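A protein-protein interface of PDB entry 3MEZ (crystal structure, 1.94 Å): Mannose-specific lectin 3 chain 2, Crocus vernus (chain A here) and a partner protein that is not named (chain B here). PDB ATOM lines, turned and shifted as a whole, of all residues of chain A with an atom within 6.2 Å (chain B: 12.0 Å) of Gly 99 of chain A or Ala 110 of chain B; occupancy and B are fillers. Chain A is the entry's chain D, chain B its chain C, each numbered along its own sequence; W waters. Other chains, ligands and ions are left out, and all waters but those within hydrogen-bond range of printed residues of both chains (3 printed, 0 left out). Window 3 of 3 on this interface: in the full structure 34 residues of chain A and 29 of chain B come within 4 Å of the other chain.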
ATOM      1  N   THR A  23       4.674   0.162 -30.961  1.00  0.00           N
ATOM      2  CA  THR A  23       4.002  -0.747 -30.050  1.00  0.00           C
ATOM      3  C   THR A  23       2.659  -0.183 -29.577  1.00  0.00           C
ATOM      4  O   THR A  23       2.550   0.975 -29.358  1.00  0.00           O
ATOM      5  CB  THR A  23       4.853  -1.078 -28.842  1.00  0.00           C
ATOM      6  OG1 THR A  23       4.267  -2.130 -28.087  1.00  0.00           O
ATOM      7  CG2 THR A  23       5.030   0.097 -28.000  1.00  0.00           C
ATOM      8  N   TYR A  26       1.505   3.551 -30.113  1.00  0.00           N
ATOM      9  CA  TYR A  26       2.651   4.425 -30.203  1.00  0.00           C
ATOM     10  C   TYR A  26       3.440   4.101 -31.458  1.00  0.00           C
ATOM     11  O   TYR A  26       3.543   2.982 -31.829  1.00  0.00           O
ATOM     12  CB  TYR A  26       3.553   4.285 -28.989  1.00  0.00           C
ATOM     13  CG  TYR A  26       2.918   4.637 -27.684  1.00  0.00           C
ATOM     14  CD1 TYR A  26       2.541   3.675 -26.822  1.00  0.00           C
ATOM     15  CD2 TYR A  26       2.701   5.933 -27.330  1.00  0.00           C
ATOM     16  CE1 TYR A  26       1.973   3.970 -25.663  1.00  0.00           C
ATOM     17  CE2 TYR A  26       2.133   6.249 -26.157  1.00  0.00           C
ATOM     18  CZ  TYR A  26       1.767   5.253 -25.326  1.00  0.00           C
ATOM     19  OH  TYR A  26       1.185   5.519 -24.195  1.00  0.00           O
ATOM     20  N   LEU A  38       7.506  10.957 -31.997  1.00  0.00           N
ATOM     21  CA  LEU A  38       6.797   9.941 -31.240  1.00  0.00           C
ATOM     22  C   LEU A  38       5.353  10.385 -31.027  1.00  0.00           C
ATOM     23  O   LEU A  38       5.121  11.355 -30.402  1.00  0.00           O
ATOM     24  CB  LEU A  38       7.482   9.676 -29.914  1.00  0.00           C
ATOM     25  CG  LEU A  38       7.379   8.376 -29.130  1.00  0.00           C
ATOM     26  CD1 LEU A  38       8.197   8.505 -27.923  1.00  0.00           C
ATOM     27  CD2 LEU A  38       5.969   8.036 -28.790  1.00  0.00           C
ATOM     28  N   VAL A  47       3.716  13.288 -28.679  1.00  0.00           N
ATOM     29  CA  VAL A  47       4.443  13.226 -27.411  1.00  0.00           C
ATOM     30  C   VAL A  47       5.841  13.823 -27.294  1.00  0.00           C
ATOM     31  O   VAL A  47       6.209  14.371 -26.279  1.00  0.00           O
ATOM     32  CB  VAL A  47       4.538  11.736 -26.947  1.00  0.00           C
ATOM     33  CG1 VAL A  47       5.367  11.598 -25.699  1.00  0.00           C
ATOM     34  CG2 VAL A  47       3.202  11.168 -26.721  1.00  0.00           C
ATOM     35  N   LEU A  95      11.079   1.328 -28.134  1.00  0.00           N
ATOM     36  CA  LEU A  95       9.816   2.019 -27.991  1.00  0.00           C
ATOM     37  C   LEU A  95       8.971   1.241 -27.005  1.00  0.00           C
ATOM     38  O   LEU A  95       8.484   0.205 -27.306  1.00  0.00           O
ATOM     39  CB  LEU A  95       9.030   2.116 -29.287  1.00  0.00           C
ATOM     40  CG  LEU A  95       8.146   3.304 -29.594  1.00  0.00           C
ATOM     41  CD1 LEU A  95       6.862   3.013 -30.364  1.00  0.00           C
ATOM     42  CD2 LEU A  95       7.934   4.237 -28.473  1.00  0.00           C
ATOM     43  N   GLN A  96       8.868   1.784 -25.811  1.00  0.00           N
ATOM     44  CA  GLN A  96       8.212   1.099 -24.713  1.00  0.00           C
ATOM     45  C   GLN A  96       6.692   1.199 -24.611  1.00  0.00           C
ATOM     46  O   GLN A  96       6.103   2.104 -25.101  1.00  0.00           O
ATOM     47  CB  GLN A  96       8.880   1.412 -23.385  1.00  0.00           C
ATOM     48  CG  GLN A  96      10.412   1.277 -23.398  1.00  0.00           C
ATOM     49  CD  GLN A  96      11.033   1.592 -22.071  1.00  0.00           C
ATOM     50  OE1 GLN A  96      10.430   2.230 -21.251  1.00  0.00           O
ATOM     51  NE2 GLN A  96      12.211   1.153 -21.876  1.00  0.00           N
ATOM     52  N   ILE A  97       6.112   0.239 -23.914  1.00  0.00           N
ATOM     53  CA  ILE A  97       4.693   0.142 -23.748  1.00  0.00           C
ATOM     54  C   ILE A  97       4.156   1.320 -22.969  1.00  0.00           C
ATOM     55  O   ILE A  97       3.021   1.602 -23.043  1.00  0.00           O
ATOM     56  CB  ILE A  97       4.243  -1.193 -23.157  1.00  0.00           C
ATOM     57  CG1 ILE A  97       4.915  -1.431 -21.839  1.00  0.00           C
ATOM     58  CG2 ILE A  97       4.542  -2.316 -24.108  1.00  0.00           C
ATOM     59  CD1 ILE A  97       4.003  -1.787 -20.811  1.00  0.00           C
ATOM     60  N   ASN A  98       5.038   1.998 -22.241  1.00  0.00           N
ATOM     61  CA  ASN A  98       4.707   3.196 -21.475  1.00  0.00           C
ATOM     62  C   ASN A  98       4.813   4.488 -22.259  1.00  0.00           C
ATOM     63  O   ASN A  98       4.728   5.538 -21.714  1.00  0.00           O
ATOM     64  CB  ASN A  98       5.529   3.317 -20.219  1.00  0.00           C
ATOM     65  CG  ASN A  98       6.890   3.876 -20.469  1.00  0.00           C
ATOM     66  OD1 ASN A  98       7.495   3.627 -21.465  1.00  0.00           O
ATOM     67  ND2 ASN A  98       7.375   4.628 -19.522  1.00  0.00           N
ATOM     68  N   GLY A  99       5.042   4.373 -23.541  1.00  0.00           N
ATOM     69  CA  GLY A  99       5.121   5.520 -24.374  1.00  0.00           C
ATOM     70  C   GLY A  99       6.425   6.278 -24.429  1.00  0.00           C
ATOM     71  O   GLY A  99       6.450   7.302 -25.010  1.00  0.00           O
ATOM     72  N   GLN A 100       7.473   5.747 -23.833  1.00  0.00           N
ATOM     73  CA  GLN A 100       8.808   6.304 -23.913  1.00  0.00           C
ATOM     74  C   GLN A 100       9.727   5.577 -24.919  1.00  0.00           C
ATOM     75  O   GLN A 100       9.721   4.391 -24.995  1.00  0.00           O
ATOM     76  CB  GLN A 100       9.497   6.193 -22.574  1.00  0.00           C
ATOM     77  CG  GLN A 100       9.227   7.199 -21.569  1.00  0.00           C
ATOM     78  CD  GLN A 100      10.115   7.045 -20.351  1.00  0.00           C
ATOM     79  OE1 GLN A 100       9.982   6.116 -19.631  1.00  0.00           O
ATOM     80  NE2 GLN A 100      11.021   7.956 -20.157  1.00  0.00           N
ATOM     81  N   ALA A 101      10.552   6.322 -25.619  1.00  0.00           N
ATOM     82  CA  ALA A 101      11.650   5.745 -26.345  1.00  0.00           C
ATOM     83  C   ALA A 101      12.911   5.928 -25.496  1.00  0.00           C
ATOM     84  O   ALA A 101      13.196   7.008 -25.035  1.00  0.00           O
ATOM     85  CB  ALA A 101      11.813   6.347 -27.672  1.00  0.00           C
ATOM     86  N   ASP B   1       5.643  -6.084 -24.648  1.00  0.00           N
ATOM     87  CA  ASP B   1       6.144  -6.840 -25.775  1.00  0.00           C
ATOM     88  C   ASP B   1       7.000  -8.047 -25.405  1.00  0.00           C
ATOM     89  O   ASP B   1       7.787  -7.973 -24.544  1.00  0.00           O
ATOM     90  CB  ASP B   1       6.799  -5.922 -26.780  1.00  0.00           C
ATOM     91  CG  ASP B   1       5.879  -4.795 -27.167  1.00  0.00           C
ATOM     92  OD1 ASP B   1       4.688  -4.889 -26.852  1.00  0.00           O
ATOM     93  OD2 ASP B   1       6.311  -3.851 -27.750  1.00  0.00           O
ATOM     94  N   VAL B   4      11.009  -8.328 -25.117  1.00  0.00           N
ATOM     95  CA  VAL B   4      11.677  -7.469 -24.155  1.00  0.00           C
ATOM     96  C   VAL B   4      11.305  -7.710 -22.675  1.00  0.00           C
ATOM     97  O   VAL B   4      10.185  -7.862 -22.368  1.00  0.00           O
ATOM     98  CB  VAL B   4      11.478  -5.973 -24.522  1.00  0.00           C
ATOM     99  CG1 VAL B   4      12.075  -5.074 -23.506  1.00  0.00           C
ATOM    100  CG2 VAL B   4      12.029  -5.704 -25.844  1.00  0.00           C
ATOM    101  N   LEU B   6      12.200  -5.638 -19.146  1.00  0.00           N
ATOM    102  CA  LEU B   6      12.791  -4.529 -18.419  1.00  0.00           C
ATOM    103  C   LEU B   6      12.970  -4.771 -16.929  1.00  0.00           C
ATOM    104  O   LEU B   6      12.273  -5.512 -16.373  1.00  0.00           O
ATOM    105  CB  LEU B   6      12.008  -3.242 -18.637  1.00  0.00           C
ATOM    106  CG  LEU B   6      11.563  -2.880 -20.051  1.00  0.00           C
ATOM    107  CD1 LEU B   6      10.792  -1.644 -20.027  1.00  0.00           C
ATOM    108  CD2 LEU B   6      12.696  -2.810 -21.002  1.00  0.00           C
ATOM    109  N   ASP B   9      10.348  -5.997 -14.041  1.00  0.00           N
ATOM    110  CA  ASP B   9       9.374  -6.909 -14.565  1.00  0.00           C
ATOM    111  C   ASP B   9       9.724  -8.371 -14.323  1.00  0.00           C
ATOM    112  O   ASP B   9      10.849  -8.693 -14.087  1.00  0.00           O
ATOM    113  CB  ASP B   9       9.072  -6.603 -16.008  1.00  0.00           C
ATOM    114  CG  ASP B   9       8.225  -5.324 -16.156  1.00  0.00           C
ATOM    115  OD1 ASP B   9       7.592  -4.893 -15.183  1.00  0.00           O
ATOM    116  OD2 ASP B   9       8.174  -4.735 -17.221  1.00  0.00           O
ATOM    117  N   TRP B 105      19.576   7.670 -22.371  1.00  0.00           N
ATOM    118  CA  TRP B 105      18.762   8.735 -22.888  1.00  0.00           C
ATOM    119  C   TRP B 105      17.331   8.221 -23.015  1.00  0.00           C
ATOM    120  O   TRP B 105      17.128   7.105 -23.343  1.00  0.00           O
ATOM    121  CB  TRP B 105      19.267   9.176 -24.250  1.00  0.00           C
ATOM    122  CG  TRP B 105      18.514  10.269 -24.957  1.00  0.00           C
ATOM    123  CD1 TRP B 105      18.777  11.571 -24.921  1.00  0.00           C
ATOM    124  CD2 TRP B 105      17.408  10.120 -25.823  1.00  0.00           C
ATOM    125  NE1 TRP B 105      17.929  12.257 -25.693  1.00  0.00           N
ATOM    126  CE2 TRP B 105      17.057  11.384 -26.255  1.00  0.00           C
ATOM    127  CE3 TRP B 105      16.659   9.049 -26.243  1.00  0.00           C
ATOM    128  CZ2 TRP B 105      16.006  11.597 -27.087  1.00  0.00           C
ATOM    129  CZ3 TRP B 105      15.631   9.268 -27.070  1.00  0.00           C
ATOM    130  CH2 TRP B 105      15.315  10.521 -27.492  1.00  0.00           C
ATOM    131  N   SER B 106      16.381   9.080 -22.743  1.00  0.00           N
ATOM    132  CA  SER B 106      15.005   8.810 -23.014  1.00  0.00           C
ATOM    133  C   SER B 106      14.158  10.037 -23.263  1.00  0.00           C
ATOM    134  O   SER B 106      14.467  11.101 -22.807  1.00  0.00           O
ATOM    135  CB  SER B 106      14.388   7.994 -21.912  1.00  0.00           C
ATOM    136  OG  SER B 106      14.422   8.689 -20.751  1.00  0.00           O
ATOM    137  N   THR B 107      13.061   9.814 -23.960  1.00  0.00           N
ATOM    138  CA  THR B 107      12.030  10.807 -24.142  1.00  0.00           C
ATOM    139  C   THR B 107      11.275  10.946 -22.834  1.00  0.00           C
ATOM    140  O   THR B 107      11.348  10.082 -22.045  1.00  0.00           O
ATOM    141  CB  THR B 107      11.086  10.466 -25.289  1.00  0.00           C
ATOM    142  OG1 THR B 107      10.446   9.236 -25.022  1.00  0.00           O
ATOM    143  CG2 THR B 107      11.853  10.392 -26.567  1.00  0.00           C
ATOM    144  N   PRO B 108      10.596  12.055 -22.604  1.00  0.00           N
ATOM    145  CA  PRO B 108       9.947  12.268 -21.311  1.00  0.00           C
ATOM    146  C   PRO B 108       8.842  11.271 -21.007  1.00  0.00           C
ATOM    147  O   PRO B 108       8.123  10.943 -21.855  1.00  0.00           O
ATOM    148  CB  PRO B 108       9.379  13.681 -21.436  1.00  0.00           C
ATOM    149  CG  PRO B 108      10.148  14.313 -22.397  1.00  0.00           C
ATOM    150  CD  PRO B 108      10.564  13.276 -23.395  1.00  0.00           C
ATOM    151  N   ALA B 109       8.716  10.820 -19.784  1.00  0.00           N
ATOM    152  CA  ALA B 109       7.569  10.032 -19.380  1.00  0.00           C
ATOM    153  C   ALA B 109       6.298  10.828 -19.579  1.00  0.00           C
ATOM    154  O   ALA B 109       6.235  11.925 -19.154  1.00  0.00           O
ATOM    155  CB  ALA B 109       7.701   9.682 -17.976  1.00  0.00           C
ATOM    156  N   ALA B 110       5.289  10.289 -20.223  1.00  0.00           N
ATOM    157  CA  ALA B 110       5.365   9.017 -20.825  1.00  0.00           C
ATOM    158  C   ALA B 110       4.667   9.090 -22.163  1.00  0.00           C
ATOM    159  O   ALA B 110       3.470   9.322 -22.232  1.00  0.00           O
ATOM    160  CB  ALA B 110       4.709   7.998 -19.944  1.00  0.00           C
HETATM  161  O   HOH W   1      13.088   7.527 -17.756  1.00  0.00           O
HETATM  162  O   HOH W   2       8.469  -2.663 -26.600  1.00  0.00           O
HETATM  163  O   HOH W   3       7.958   9.865 -24.604  1.00  0.00           O
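N of Ala 101 of chain A sits at hydrogen-bond distance from OG1 of Thr 107 of chain B (3.0 Å).
O of Thr 107 of chain B lies within hydrogen-bond range of NE2 of Gln 100 of chain A.
OG1 of Thr 23 of chain A sits at hydrogen-bond distance from OD2 of Asp 1 of chain B (2.7 Å).
The backbone carbonyl oxygen (O) of Leu 38 of chain A sits at hydrogen-bond distance from the backbone NH (N) of Val 47 of chain A (2.9 Å).
OE1 of Gln 96 of chain A sits close to OD1 of Asn 98 of chain A (3.3 Å).
The side-chain amide oxygen (OE1) of Gln 100 of chain A is in hydrogen-bond range of the side-chain amide nitrogen (ND2) of Asn 98 of chain A.
Among the printed residues, pairs that only touch across the chains: Asn 98 of chain A with Ala 110 of chain B (3.0 Å), Ala 101 of chain A with Ser 106 of chain B (3.3 Å), Gln 100 of chain A with Ser 106 of chain B (3.5 Å), Gln 96 of chain A with Leu 6 of chain B (3.6 Å), Gln 100 of chain A with Ala 109 of chain B (3.7 Å), Leu 38 of chain A with Thr 107 of chain B (3.7 Å), Ile 97 of chain A with Asp 1 of chain B (3.8 Å), Gly 99 of chain A with Ala 110 of chain B (3.8 Å), Ala 101 of chain A with Trp 105 of chain B (3.9 Å) and Gln 100 of chain A with Pro 108 of chain B (3.9 Å).
No residue of chain B comes within 4 Å of Leu 95 of chain A.
Of chain B, only Asp 1 comes within 4 Å of Ile 97 of chain A.
Gln 100 of chain A touches four residues of chain B.
Asp 9 of chain B touches none of the printed residues of chain A.
Of the printed residues of chain A, Ser 106 of chain B touches Gln 100 (3.5 Å) and Ala 101 (3.3 Å).
Of the printed residues of chain A, Pro 108 of chain B touches Gln 100 (3.9 Å).
Ala 110 of chain B touches just these residues of chain A: Asn 98 and Gly 99.
The nearest residue of chain A that does not touch Ala 110 of chain B is Gln 100 of chain A (4.3 Å).
Printed residues of chain A that touch a printed residue of chain B: Thr 23, Leu 38, Gln 96, Ile 97, Asn 98, Gly 99, Gln 100 and Ala 101.
Of the 10 printed residues of chain B, 8 touch a printed residue of chain A.
Printed residues of chain B that touch a printed residue of chain A: Asp 1, Leu 6, Trp 105, Ser 106, Thr 107, Pro 108, Ala 109 and Ala 110.
Among the printed residues, 13 pairs touch across the chains.
Among the printed residues, no Asp or Glu carboxylate lies within 4 Å of a Lys or Arg side-chain nitrogen of the other chain.
Water W3 lies within hydrogen-bond range of OG1 of Thr 107 of chain B (2.6 Å), O of Pro 108 of chain B (3.0 Å) and O of Gly 99 of chain A (3.0 Å).
Water W2 bridges OD2 of Asp 1 of chain B (2.7 Å) and O of Leu 95 of chain A (3.0 Å).
Water W1 bridges NE2 of Gln 100 of chain A and OG of Ser 106 of chain B.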
